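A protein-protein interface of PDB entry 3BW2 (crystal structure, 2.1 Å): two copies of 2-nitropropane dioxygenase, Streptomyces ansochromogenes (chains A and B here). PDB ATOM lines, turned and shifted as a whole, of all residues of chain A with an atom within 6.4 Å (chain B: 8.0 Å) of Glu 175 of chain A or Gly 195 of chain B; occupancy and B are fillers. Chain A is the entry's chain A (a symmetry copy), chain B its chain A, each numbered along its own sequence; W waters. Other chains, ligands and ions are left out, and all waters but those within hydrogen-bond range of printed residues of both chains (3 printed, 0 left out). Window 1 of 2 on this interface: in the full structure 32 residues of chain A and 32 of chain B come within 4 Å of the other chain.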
ATOM      1  N   GLN A 172      22.646  -1.896  -7.581  1.00  0.00           N
ATOM      2  CA  GLN A 172      22.669  -1.339  -6.237  1.00  0.00           C
ATOM      3  C   GLN A 172      21.622  -0.239  -6.086  1.00  0.00           C
ATOM      4  O   GLN A 172      21.719   0.813  -6.719  1.00  0.00           O
ATOM      5  CB  GLN A 172      24.061  -0.782  -5.930  1.00  0.00           C
ATOM      6  CG  GLN A 172      24.189  -0.139  -4.557  1.00  0.00           C
ATOM      7  CD  GLN A 172      25.383   0.785  -4.480  1.00  0.00           C
ATOM      8  OE1 GLN A 172      25.584   1.622  -5.364  1.00  0.00           O
ATOM      9  NE2 GLN A 172      26.181   0.650  -3.418  1.00  0.00           N
ATOM     10  N   GLY A 173      20.630  -0.494  -5.236  1.00  0.00           N
ATOM     11  CA  GLY A 173      19.565   0.469  -5.014  1.00  0.00           C
ATOM     12  C   GLY A 173      19.944   1.619  -4.099  1.00  0.00           C
ATOM     13  O   GLY A 173      21.016   1.626  -3.487  1.00  0.00           O
ATOM     14  N   VAL A 174      19.045   2.591  -3.990  1.00  0.00           N
ATOM     15  CA  VAL A 174      19.288   3.767  -3.165  1.00  0.00           C
ATOM     16  C   VAL A 174      19.408   3.432  -1.675  1.00  0.00           C
ATOM     17  O   VAL A 174      20.038   4.174  -0.916  1.00  0.00           O
ATOM     18  CB  VAL A 174      18.163   4.821  -3.376  1.00  0.00           C
ATOM     19  CG1 VAL A 174      16.888   4.376  -2.682  1.00  0.00           C
ATOM     20  CG2 VAL A 174      18.613   6.177  -2.874  1.00  0.00           C
ATOM     21  N   GLU A 175      18.822   2.312  -1.259  1.00  0.00           N
ATOM     22  CA  GLU A 175      18.852   1.903   0.149  1.00  0.00           C
ATOM     23  C   GLU A 175      20.218   1.425   0.644  1.00  0.00           C
ATOM     24  O   GLU A 175      20.459   1.361   1.850  1.00  0.00           O
ATOM     25  CB  GLU A 175      17.839   0.779   0.399  1.00  0.00           C
ATOM     26  CG  GLU A 175      16.423   1.081  -0.070  1.00  0.00           C
ATOM     27  CD  GLU A 175      16.125   0.472  -1.424  1.00  0.00           C
ATOM     28  OE1 GLU A 175      16.870   0.752  -2.385  1.00  0.00           O
ATOM     29  OE2 GLU A 175      15.144  -0.290  -1.521  1.00  0.00           O
ATOM     30  N   ALA A 176      21.092   1.079  -0.296  1.00  0.00           N
ATOM     31  CA  ALA A 176      22.432   0.573   0.004  1.00  0.00           C
ATOM     32  C   ALA A 176      23.270   1.403   0.976  1.00  0.00           C
ATOM     33  O   ALA A 176      23.191   2.633   1.004  1.00  0.00           O
ATOM     34  CB  ALA A 176      23.209   0.392  -1.304  1.00  0.00           C
ATOM     35  N   GLY A 177      24.083   0.712   1.767  1.00  0.00           N
ATOM     36  CA  GLY A 177      24.965   1.396   2.693  1.00  0.00           C
ATOM     37  C   GLY A 177      26.278   1.670   1.975  1.00  0.00           C
ATOM     38  O   GLY A 177      26.587   1.019   0.972  1.00  0.00           O
ATOM     39  N   GLN A 180      27.497   4.944  -3.242  1.00  0.00           N
ATOM     40  CA  GLN A 180      26.629   4.639  -4.365  1.00  0.00           C
ATOM     41  C   GLN A 180      27.626   4.385  -5.489  1.00  0.00           C
ATOM     42  O   GLN A 180      28.574   5.158  -5.657  1.00  0.00           O
ATOM     43  CB  GLN A 180      25.756   5.845  -4.711  1.00  0.00           C
ATOM     44  CG  GLN A 180      24.513   5.974  -3.853  1.00  0.00           C
ATOM     45  CD  GLN A 180      23.536   4.847  -4.110  1.00  0.00           C
ATOM     46  OE1 GLN A 180      23.329   3.979  -3.260  1.00  0.00           O
ATOM     47  NE2 GLN A 180      22.937   4.845  -5.298  1.00  0.00           N
ATOM     48  N   ILE A 194      17.308   5.418  -7.146  1.00  0.00           N
ATOM     49  CA  ILE A 194      16.201   4.505  -7.410  1.00  0.00           C
ATOM     50  C   ILE A 194      16.072   3.361  -6.393  1.00  0.00           C
ATOM     51  O   ILE A 194      17.056   2.683  -6.082  1.00  0.00           O
ATOM     52  CB  ILE A 194      16.349   3.893  -8.820  1.00  0.00           C
ATOM     53  CG1 ILE A 194      16.505   5.018  -9.852  1.00  0.00           C
ATOM     54  CG2 ILE A 194      15.140   3.025  -9.149  1.00  0.00           C
ATOM     55  CD1 ILE A 194      16.858   4.534 -11.235  1.00  0.00           C
ATOM     56  N   GLY A 195      14.855   3.152  -5.885  1.00  0.00           N
ATOM     57  CA  GLY A 195      14.621   2.072  -4.936  1.00  0.00           C
ATOM     58  C   GLY A 195      15.012   0.757  -5.582  1.00  0.00           C
ATOM     59  O   GLY A 195      14.754   0.555  -6.770  1.00  0.00           O
ATOM     60  N   LEU A 196      15.623  -0.143  -4.815  1.00  0.00           N
ATOM     61  CA  LEU A 196      16.075  -1.424  -5.358  1.00  0.00           C
ATOM     62  C   LEU A 196      15.032  -2.224  -6.136  1.00  0.00           C
ATOM     63  O   LEU A 196      15.322  -2.726  -7.222  1.00  0.00           O
ATOM     64  CB  LEU A 196      16.649  -2.311  -4.244  1.00  0.00           C
ATOM     65  CG  LEU A 196      17.207  -3.668  -4.702  1.00  0.00           C
ATOM     66  CD1 LEU A 196      18.327  -3.455  -5.740  1.00  0.00           C
ATOM     67  CD2 LEU A 196      17.742  -4.434  -3.493  1.00  0.00           C
ATOM     68  N   LEU A 197      13.826  -2.361  -5.587  1.00  0.00           N
ATOM     69  CA  LEU A 197      12.787  -3.138  -6.263  1.00  0.00           C
ATOM     70  C   LEU A 197      12.478  -2.581  -7.651  1.00  0.00           C
ATOM     71  O   LEU A 197      12.172  -3.329  -8.584  1.00  0.00           O
ATOM     72  CB  LEU A 197      11.507  -3.181  -5.415  1.00  0.00           C
ATOM     73  CG  LEU A 197      10.346  -4.012  -5.975  1.00  0.00           C
ATOM     74  CD1 LEU A 197      10.805  -5.439  -6.244  1.00  0.00           C
ATOM     75  CD2 LEU A 197       9.190  -4.007  -4.984  1.00  0.00           C
ATOM     76  N   ALA A 214      21.468  -5.468  -4.719  1.00  0.00           N
ATOM     77  CA  ALA A 214      22.110  -4.950  -3.514  1.00  0.00           C
ATOM     78  C   ALA A 214      21.435  -3.699  -2.950  1.00  0.00           C
ATOM     79  O   ALA A 214      21.060  -2.783  -3.696  1.00  0.00           O
ATOM     80  CB  ALA A 214      23.577  -4.650  -3.798  1.00  0.00           C
ATOM     81  N   GLY A 215      21.297  -3.662  -1.627  1.00  0.00           N
ATOM     82  CA  GLY A 215      20.697  -2.510  -0.976  1.00  0.00           C
ATOM     83  C   GLY A 215      19.579  -2.795   0.010  1.00  0.00           C
ATOM     84  O   GLY A 215      18.469  -3.118  -0.389  1.00  0.00           O
ATOM     85  N   GLY A 216      19.878  -2.674   1.301  1.00  0.00           N
ATOM     86  CA  GLY A 216      18.879  -2.893   2.336  1.00  0.00           C
ATOM     87  C   GLY A 216      18.453  -4.323   2.633  1.00  0.00           C
ATOM     88  O   GLY A 216      17.520  -4.532   3.411  1.00  0.00           O
ATOM     89  N   THR A 264      19.471   7.174   8.401  1.00  0.00           N
ATOM     90  CA  THR A 264      20.617   7.248   7.512  1.00  0.00           C
ATOM     91  C   THR A 264      20.330   8.283   6.435  1.00  0.00           C
ATOM     92  O   THR A 264      19.177   8.671   6.214  1.00  0.00           O
ATOM     93  CB  THR A 264      20.883   5.908   6.805  1.00  0.00           C
ATOM     94  OG1 THR A 264      19.840   5.654   5.855  1.00  0.00           O
ATOM     95  CG2 THR A 264      20.925   4.771   7.810  1.00  0.00           C
ATOM     96  N   ARG A 276      25.834   6.386   1.844  1.00  0.00           N
ATOM     97  CA  ARG A 276      24.847   6.332   2.924  1.00  0.00           C
ATOM     98  C   ARG A 276      25.464   5.971   4.272  1.00  0.00           C
ATOM     99  O   ARG A 276      26.064   4.904   4.441  1.00  0.00           O
ATOM    100  CB  ARG A 276      23.732   5.343   2.572  1.00  0.00           C
ATOM    101  CG  ARG A 276      22.608   5.287   3.604  1.00  0.00           C
ATOM    102  CD  ARG A 276      21.498   4.351   3.157  1.00  0.00           C
ATOM    103  NE  ARG A 276      20.809   4.842   1.966  1.00  0.00           N
ATOM    104  CZ  ARG A 276      19.952   5.861   1.950  1.00  0.00           C
ATOM    105  NH1 ARG A 276      19.658   6.517   3.066  1.00  0.00           N
ATOM    106  NH2 ARG A 276      19.384   6.227   0.809  1.00  0.00           N
ATOM    107  N   ALA A 321      26.050   2.545   6.375  1.00  0.00           N
ATOM    108  CA  ALA A 321      24.985   1.610   6.722  1.00  0.00           C
ATOM    109  C   ALA A 321      23.801   1.765   5.774  1.00  0.00           C
ATOM    110  O   ALA A 321      23.458   2.880   5.381  1.00  0.00           O
ATOM    111  CB  ALA A 321      24.532   1.845   8.171  1.00  0.00           C
ATOM    112  N   GLY A 322      23.193   0.641   5.404  1.00  0.00           N
ATOM    113  CA  GLY A 322      22.043   0.674   4.520  1.00  0.00           C
ATOM    114  C   GLY A 322      20.807   0.997   5.339  1.00  0.00           C
ATOM    115  O   GLY A 322      20.864   1.003   6.569  1.00  0.00           O
ATOM    116  N   GLN A 323      19.688   1.256   4.672  1.00  0.00           N
ATOM    117  CA  GLN A 323      18.457   1.603   5.371  1.00  0.00           C
ATOM    118  C   GLN A 323      17.888   0.499   6.262  1.00  0.00           C
ATOM    119  O   GLN A 323      16.993   0.749   7.063  1.00  0.00           O
ATOM    120  CB  GLN A 323      17.402   2.056   4.366  1.00  0.00           C
ATOM    121  CG  GLN A 323      17.789   3.321   3.613  1.00  0.00           C
ATOM    122  CD  GLN A 323      16.647   3.860   2.781  1.00  0.00           C
ATOM    123  OE1 GLN A 323      16.028   3.123   2.021  1.00  0.00           O
ATOM    124  NE2 GLN A 323      16.361   5.152   2.922  1.00  0.00           N
ATOM    125  N   GLY A 324      18.408  -0.716   6.125  1.00  0.00           N
ATOM    126  CA  GLY A 324      17.930  -1.815   6.948  1.00  0.00           C
ATOM    127  C   GLY A 324      18.823  -2.076   8.152  1.00  0.00           C
ATOM    128  O   GLY A 324      18.730  -3.129   8.785  1.00  0.00           O
ATOM    129  N   THR B 153       4.848   5.345   6.005  1.00  0.00           N
ATOM    130  CA  THR B 153       6.091   5.396   5.240  1.00  0.00           C
ATOM    131  C   THR B 153       7.309   4.973   6.069  1.00  0.00           C
ATOM    132  O   THR B 153       8.426   4.897   5.550  1.00  0.00           O
ATOM    133  CB  THR B 153       6.333   6.811   4.661  1.00  0.00           C
ATOM    134  OG1 THR B 153       6.511   7.747   5.728  1.00  0.00           O
ATOM    135  CG2 THR B 153       5.137   7.248   3.806  1.00  0.00           C
ATOM    136  N   ALA B 171       2.268  -0.035   3.151  1.00  0.00           N
ATOM    137  CA  ALA B 171       3.660   0.389   3.261  1.00  0.00           C
ATOM    138  C   ALA B 171       4.047   1.005   1.925  1.00  0.00           C
ATOM    139  O   ALA B 171       4.312   0.295   0.955  1.00  0.00           O
ATOM    140  CB  ALA B 171       4.562  -0.810   3.586  1.00  0.00           C
ATOM    141  N   GLN B 172       4.060   2.331   1.882  1.00  0.00           N
ATOM    142  CA  GLN B 172       4.392   3.053   0.663  1.00  0.00           C
ATOM    143  C   GLN B 172       5.860   3.471   0.661  1.00  0.00           C
ATOM    144  O   GLN B 172       6.282   4.292   1.477  1.00  0.00           O
ATOM    145  CB  GLN B 172       3.497   4.287   0.532  1.00  0.00           C
ATOM    146  CG  GLN B 172       3.783   5.140  -0.695  1.00  0.00           C
ATOM    147  CD  GLN B 172       3.234   6.540  -0.546  1.00  0.00           C
ATOM    148  OE1 GLN B 172       3.444   7.188   0.484  1.00  0.00           O
ATOM    149  NE2 GLN B 172       2.533   7.026  -1.573  1.00  0.00           N
ATOM    150  N   GLY B 173       6.624   2.903  -0.269  1.00  0.00           N
ATOM    151  CA  GLY B 173       8.041   3.210  -0.367  1.00  0.00           C
ATOM    152  C   GLY B 173       8.348   4.535  -1.041  1.00  0.00           C
ATOM    153  O   GLY B 173       7.462   5.198  -1.587  1.00  0.00           O
ATOM    154  N   VAL B 174       9.621   4.913  -1.018  1.00  0.00           N
ATOM    155  CA  VAL B 174      10.054   6.174  -1.604  1.00  0.00           C
ATOM    156  C   VAL B 174       9.855   6.222  -3.123  1.00  0.00           C
ATOM    157  O   VAL B 174       9.730   7.304  -3.702  1.00  0.00           O
ATOM    158  CB  VAL B 174      11.548   6.449  -1.263  1.00  0.00           C
ATOM    159  CG1 VAL B 174      12.450   5.549  -2.088  1.00  0.00           C
ATOM    160  CG2 VAL B 174      11.878   7.908  -1.490  1.00  0.00           C
ATOM    161  N   GLU B 175       9.806   5.057  -3.762  1.00  0.00           N
ATOM    162  CA  GLU B 175       9.643   4.981  -5.217  1.00  0.00           C
ATOM    163  C   GLU B 175       8.251   5.365  -5.721  1.00  0.00           C
ATOM    164  O   GLU B 175       8.071   5.651  -6.905  1.00  0.00           O
ATOM    165  CB  GLU B 175       9.951   3.564  -5.715  1.00  0.00           C
ATOM    166  CG  GLU B 175      11.297   3.011  -5.272  1.00  0.00           C
ATOM    167  CD  GLU B 175      11.175   2.102  -4.066  1.00  0.00           C
ATOM    168  OE1 GLU B 175      10.630   2.546  -3.034  1.00  0.00           O
ATOM    169  OE2 GLU B 175      11.623   0.944  -4.157  1.00  0.00           O
ATOM    170  N   ALA B 192      14.873  11.350   3.547  1.00  0.00           N
ATOM    171  CA  ALA B 192      14.713  10.270   4.513  1.00  0.00           C
ATOM    172  C   ALA B 192      13.863   9.119   3.973  1.00  0.00           C
ATOM    173  O   ALA B 192      13.645   8.127   4.669  1.00  0.00           O
ATOM    174  CB  ALA B 192      14.094  10.817   5.801  1.00  0.00           C
ATOM    175  N   GLY B 193      13.388   9.254   2.735  1.00  0.00           N
ATOM    176  CA  GLY B 193      12.560   8.222   2.127  1.00  0.00           C
ATOM    177  C   GLY B 193      13.174   6.832   2.093  1.00  0.00           C
ATOM    178  O   GLY B 193      14.317   6.654   1.679  1.00  0.00           O
ATOM    179  N   ILE B 194      12.397   5.835   2.505  1.00  0.00           N
ATOM    180  CA  ILE B 194      12.869   4.455   2.545  1.00  0.00           C
ATOM    181  C   ILE B 194      12.447   3.611   1.334  1.00  0.00           C
ATOM    182  O   ILE B 194      11.271   3.598   0.955  1.00  0.00           O
ATOM    183  CB  ILE B 194      12.359   3.762   3.827  1.00  0.00           C
ATOM    184  CG1 ILE B 194      12.748   4.602   5.051  1.00  0.00           C
ATOM    185  CG2 ILE B 194      12.938   2.356   3.934  1.00  0.00           C
ATOM    186  CD1 ILE B 194      12.129   4.126   6.340  1.00  0.00           C
ATOM    187  N   GLY B 195      13.410   2.905   0.736  1.00  0.00           N
ATOM    188  CA  GLY B 195      13.107   2.048  -0.403  1.00  0.00           C
ATOM    189  C   GLY B 195      12.068   1.026   0.015  1.00  0.00           C
ATOM    190  O   GLY B 195      12.128   0.511   1.133  1.00  0.00           O
ATOM    191  N   LEU B 196      11.122   0.719  -0.870  1.00  0.00           N
ATOM    192  CA  LEU B 196      10.053  -0.225  -0.545  1.00  0.00           C
ATOM    193  C   LEU B 196      10.502  -1.570   0.023  1.00  0.00           C
ATOM    194  O   LEU B 196       9.943  -2.040   1.015  1.00  0.00           O
ATOM    195  CB  LEU B 196       9.163  -0.478  -1.771  1.00  0.00           C
ATOM    196  CG  LEU B 196       7.970  -1.416  -1.536  1.00  0.00           C
ATOM    197  CD1 LEU B 196       7.065  -0.853  -0.422  1.00  0.00           C
ATOM    198  CD2 LEU B 196       7.180  -1.570  -2.835  1.00  0.00           C
ATOM    199  N   LEU B 197      11.495  -2.203  -0.600  1.00  0.00           N
ATOM    200  CA  LEU B 197      11.957  -3.508  -0.129  1.00  0.00           C
ATOM    201  C   LEU B 197      12.437  -3.447   1.320  1.00  0.00           C
ATOM    202  O   LEU B 197      12.271  -4.401   2.087  1.00  0.00           O
ATOM    203  CB  LEU B 197      13.076  -4.045  -1.032  1.00  0.00           C
ATOM    204  CG  LEU B 197      13.621  -5.437  -0.690  1.00  0.00           C
ATOM    205  CD1 LEU B 197      12.485  -6.451  -0.660  1.00  0.00           C
ATOM    206  CD2 LEU B 197      14.665  -5.844  -1.721  1.00  0.00           C
ATOM    207  N   SER B 198      13.029  -2.322   1.695  1.00  0.00           N
ATOM    208  CA  SER B 198      13.517  -2.163   3.052  1.00  0.00           C
ATOM    209  C   SER B 198      12.349  -1.810   3.980  1.00  0.00           C
ATOM    210  O   SER B 198      12.207  -2.379   5.064  1.00  0.00           O
ATOM    211  CB  SER B 198      14.589  -1.074   3.094  1.00  0.00           C
ATOM    212  OG  SER B 198      15.172  -0.999   4.379  1.00  0.00           O
ATOM    213  N   LEU B 199      11.502  -0.882   3.545  1.00  0.00           N
ATOM    214  CA  LEU B 199      10.352  -0.480   4.350  1.00  0.00           C
ATOM    215  C   LEU B 199       9.433  -1.667   4.639  1.00  0.00           C
ATOM    216  O   LEU B 199       8.945  -1.831   5.761  1.00  0.00           O
ATOM    217  CB  LEU B 199       9.549   0.620   3.640  1.00  0.00           C
ATOM    218  CG  LEU B 199       8.254   1.042   4.351  1.00  0.00           C
ATOM    219  CD1 LEU B 199       8.579   1.589   5.746  1.00  0.00           C
ATOM    220  CD2 LEU B 199       7.526   2.090   3.521  1.00  0.00           C
ATOM    221  N   LEU B 200       9.190  -2.486   3.622  1.00  0.00           N
ATOM    222  CA  LEU B 200       8.322  -3.649   3.781  1.00  0.00           C
ATOM    223  C   LEU B 200       8.806  -4.588   4.883  1.00  0.00           C
ATOM    224  O   LEU B 200       8.024  -5.008   5.737  1.00  0.00           O
ATOM    225  CB  LEU B 200       8.212  -4.416   2.461  1.00  0.00           C
ATOM    226  CG  LEU B 200       7.378  -5.698   2.494  1.00  0.00           C
ATOM    227  CD1 LEU B 200       5.984  -5.407   3.048  1.00  0.00           C
ATOM    228  CD2 LEU B 200       7.284  -6.273   1.089  1.00  0.00           C
ATOM    229  N   ALA B 201      10.097  -4.907   4.866  1.00  0.00           N
ATOM    230  CA  ALA B 201      10.666  -5.803   5.867  1.00  0.00           C
ATOM    231  C   ALA B 201      10.554  -5.211   7.266  1.00  0.00           C
ATOM    232  O   ALA B 201      10.223  -5.915   8.222  1.00  0.00           O
ATOM    233  CB  ALA B 201      12.131  -6.100   5.535  1.00  0.00           C
ATOM    234  N   GLN B 202      10.831  -3.914   7.383  1.00  0.00           N
ATOM    235  CA  GLN B 202      10.759  -3.224   8.667  1.00  0.00           C
ATOM    236  C   GLN B 202       9.325  -3.208   9.201  1.00  0.00           C
ATOM    237  O   GLN B 202       9.087  -3.484  10.377  1.00  0.00           O
ATOM    238  CB  GLN B 202      11.260  -1.781   8.532  1.00  0.00           C
ATOM    239  CG  GLN B 202      12.751  -1.628   8.239  1.00  0.00           C
ATOM    240  CD  GLN B 202      13.163  -0.167   8.117  1.00  0.00           C
ATOM    241  OE1 GLN B 202      13.003   0.618   9.054  1.00  0.00           O
ATOM    242  NE2 GLN B 202      13.690   0.205   6.958  1.00  0.00           N
ATOM    243  N   ALA B 214       3.392  -0.759  -1.631  1.00  0.00           N
ATOM    244  CA  ALA B 214       3.165   0.221  -2.690  1.00  0.00           C
ATOM    245  C   ALA B 214       4.411   1.031  -3.053  1.00  0.00           C
ATOM    246  O   ALA B 214       5.164   1.475  -2.173  1.00  0.00           O
ATOM    247  CB  ALA B 214       2.044   1.172  -2.283  1.00  0.00           C
ATOM    248  N   GLY B 215       4.615   1.230  -4.352  1.00  0.00           N
ATOM    249  CA  GLY B 215       5.750   2.010  -4.814  1.00  0.00           C
ATOM    250  C   GLY B 215       6.613   1.376  -5.890  1.00  0.00           C
ATOM    251  O   GLY B 215       7.382   0.467  -5.610  1.00  0.00           O
ATOM    252  N   GLN B 323       8.820   5.678  -9.736  1.00  0.00           N
ATOM    253  CA  GLN B 323      10.089   5.467 -10.421  1.00  0.00           C
ATOM    254  C   GLN B 323      10.059   4.408 -11.522  1.00  0.00           C
ATOM    255  O   GLN B 323      10.995   4.306 -12.310  1.00  0.00           O
ATOM    256  CB  GLN B 323      11.176   5.129  -9.405  1.00  0.00           C
ATOM    257  CG  GLN B 323      11.452   6.254  -8.417  1.00  0.00           C
ATOM    258  CD  GLN B 323      12.666   5.975  -7.561  1.00  0.00           C
ATOM    259  OE1 GLN B 323      12.783   4.902  -6.977  1.00  0.00           O
ATOM    260  NE2 GLN B 323      13.578   6.941  -7.480  1.00  0.00           N
HETATM  261  O   HOH W   1      15.849  -2.577   0.297  1.00  0.00           O
HETATM  262  O   HOH W   2      15.354   2.866   7.250  1.00  0.00           O
HETATM  263  O   HOH W   3      15.772  -3.497   5.172  1.00  0.00           O
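Glu 175 of chain A touches Gly 195 of chain B, and with the chains exchanged Gly 195 of chain A touches Glu 175 of chain B. Ile 194 of chain A touches Gln 323 of chain B, and with the chains exchanged Gln 323 of chain A touches Ile 194 of chain B. Gly 195 of chain A touches Gln 323 of chain B, and with the chains exchanged Gln 323 of chain A touches Gly 195 of chain B. Leu 196 of chain A touches Leu 197 of chain B, and with the chains exchanged Leu 197 of chain A touches Leu 196 of chain B. Of the 12 pairs that touch across the chains among the printed residues, 8 have their exchanged pair printed and touching as well.
N of Val 174 of chain B lies within hydrogen-bond range of O of Ile 194 of chain B, at 2.9 Å. The side-chain carboxylate (OE1) of Glu 175 of chain B sits at hydrogen-bond distance from the backbone NH (N) of Leu 196 of chain B, at 2.9 Å. N of Gln 323 of chain B lies within hydrogen-bond range of O of Glu 175 of chain B, 2.9 Å away. The side-chain hydroxyl (OG) of Ser 198 of chain B sits at hydrogen-bond distance from the side-chain amide nitrogen (NE2) of Gln 202 of chain B (3.2 Å). The side-chain carboxylate of Glu 175 of chain A sits at hydrogen-bond distance from the backbone NH of Leu 196 of chain A. The backbone carbonyl oxygen (O) of Glu 175 of chain A sits at hydrogen-bond distance from the backbone NH (N) of Gln 323 of chain A, 2.9 Å away.
Glu 175 of chain A touches one residue of chain B. No residue of chain B comes within 4 Å of Ala 176 of chain A. Of the printed residues of chain A, Glu 175 of chain B touches Gly 195. Gly 195 of chain B touches just these residues of chain A: Glu 175 and Gln 323. Printed residues of chain A within 4 Å of Leu 196 of chain B: Leu 197 (3.8 Å). The nearest printed residue of chain A that does not touch Gln 323 of chain B is Val 174 of chain A (6.0 Å).
Printed residues of chain B that touch a printed residue of chain A: Glu 175, Gly 193, Ile 194, Gly 195, Leu 196, Leu 197, Ser 198, Gln 202 and Gln 323. Hydrophobic or aromatic side chains of chain B that line the printed part of chain A: Ile 194, Leu 196 and Leu 197.
Glu 175 of chain A touches Gly 195 of chain B (OE2 to CA, 3.3 Å). CA of Ile 194 of chain A touches OE1 of Gln 323 of chain B, 3.5 Å away. CA of Gly 195 of chain A touches OE2 of Glu 175 of chain B, 3.3 Å away. Leu 197 of chain B touches Leu 196 of chain A. Leu 197 of chain A touches Leu 196 of chain B. Ile 194 of chain B touches Gln 323 of chain A. Ser 198 of chain B touches Gln 323 of chain A. N of Gly 324 of chain A touches OG of Ser 198 of chain B, at 3.7 Å.
NE2 of Gln 323 of chain A is in hydrogen-bond range of O of Gly 193 of chain B. The backbone NH (N) of Gly 195 of chain B is in hydrogen-bond range of the side-chain amide oxygen (OE1) of Gln 323 of chain A (2.9 Å). The side-chain amide nitrogen (NE2) of Gln 202 of chain B is in hydrogen-bond range of the backbone carbonyl oxygen (O) of Gln 323 of chain A, at 3.3 Å. The backbone NH (N) of Gly 195 of chain A is in hydrogen-bond range of the side-chain amide oxygen (OE1) of Gln 323 of chain B (2.9 Å).
Water W2 bridges the backbone carbonyl oxygen of Gln 323 of chain A and the side-chain amide nitrogen of Gln 202 of chain B. Water W3 bridges the backbone carbonyl oxygen (O) of Gly 216 of chain A and the side-chain hydroxyl (OG) of Ser 198 of chain B. Water W1 lies within hydrogen-bond range of the backbone carbonyl oxygen of Gly 215 of chain A (2.8 Å), the side-chain carboxylate of Glu 175 of chain A (3.0 Å) and the backbone NH of Ser 198 of chain B (3.2 Å).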
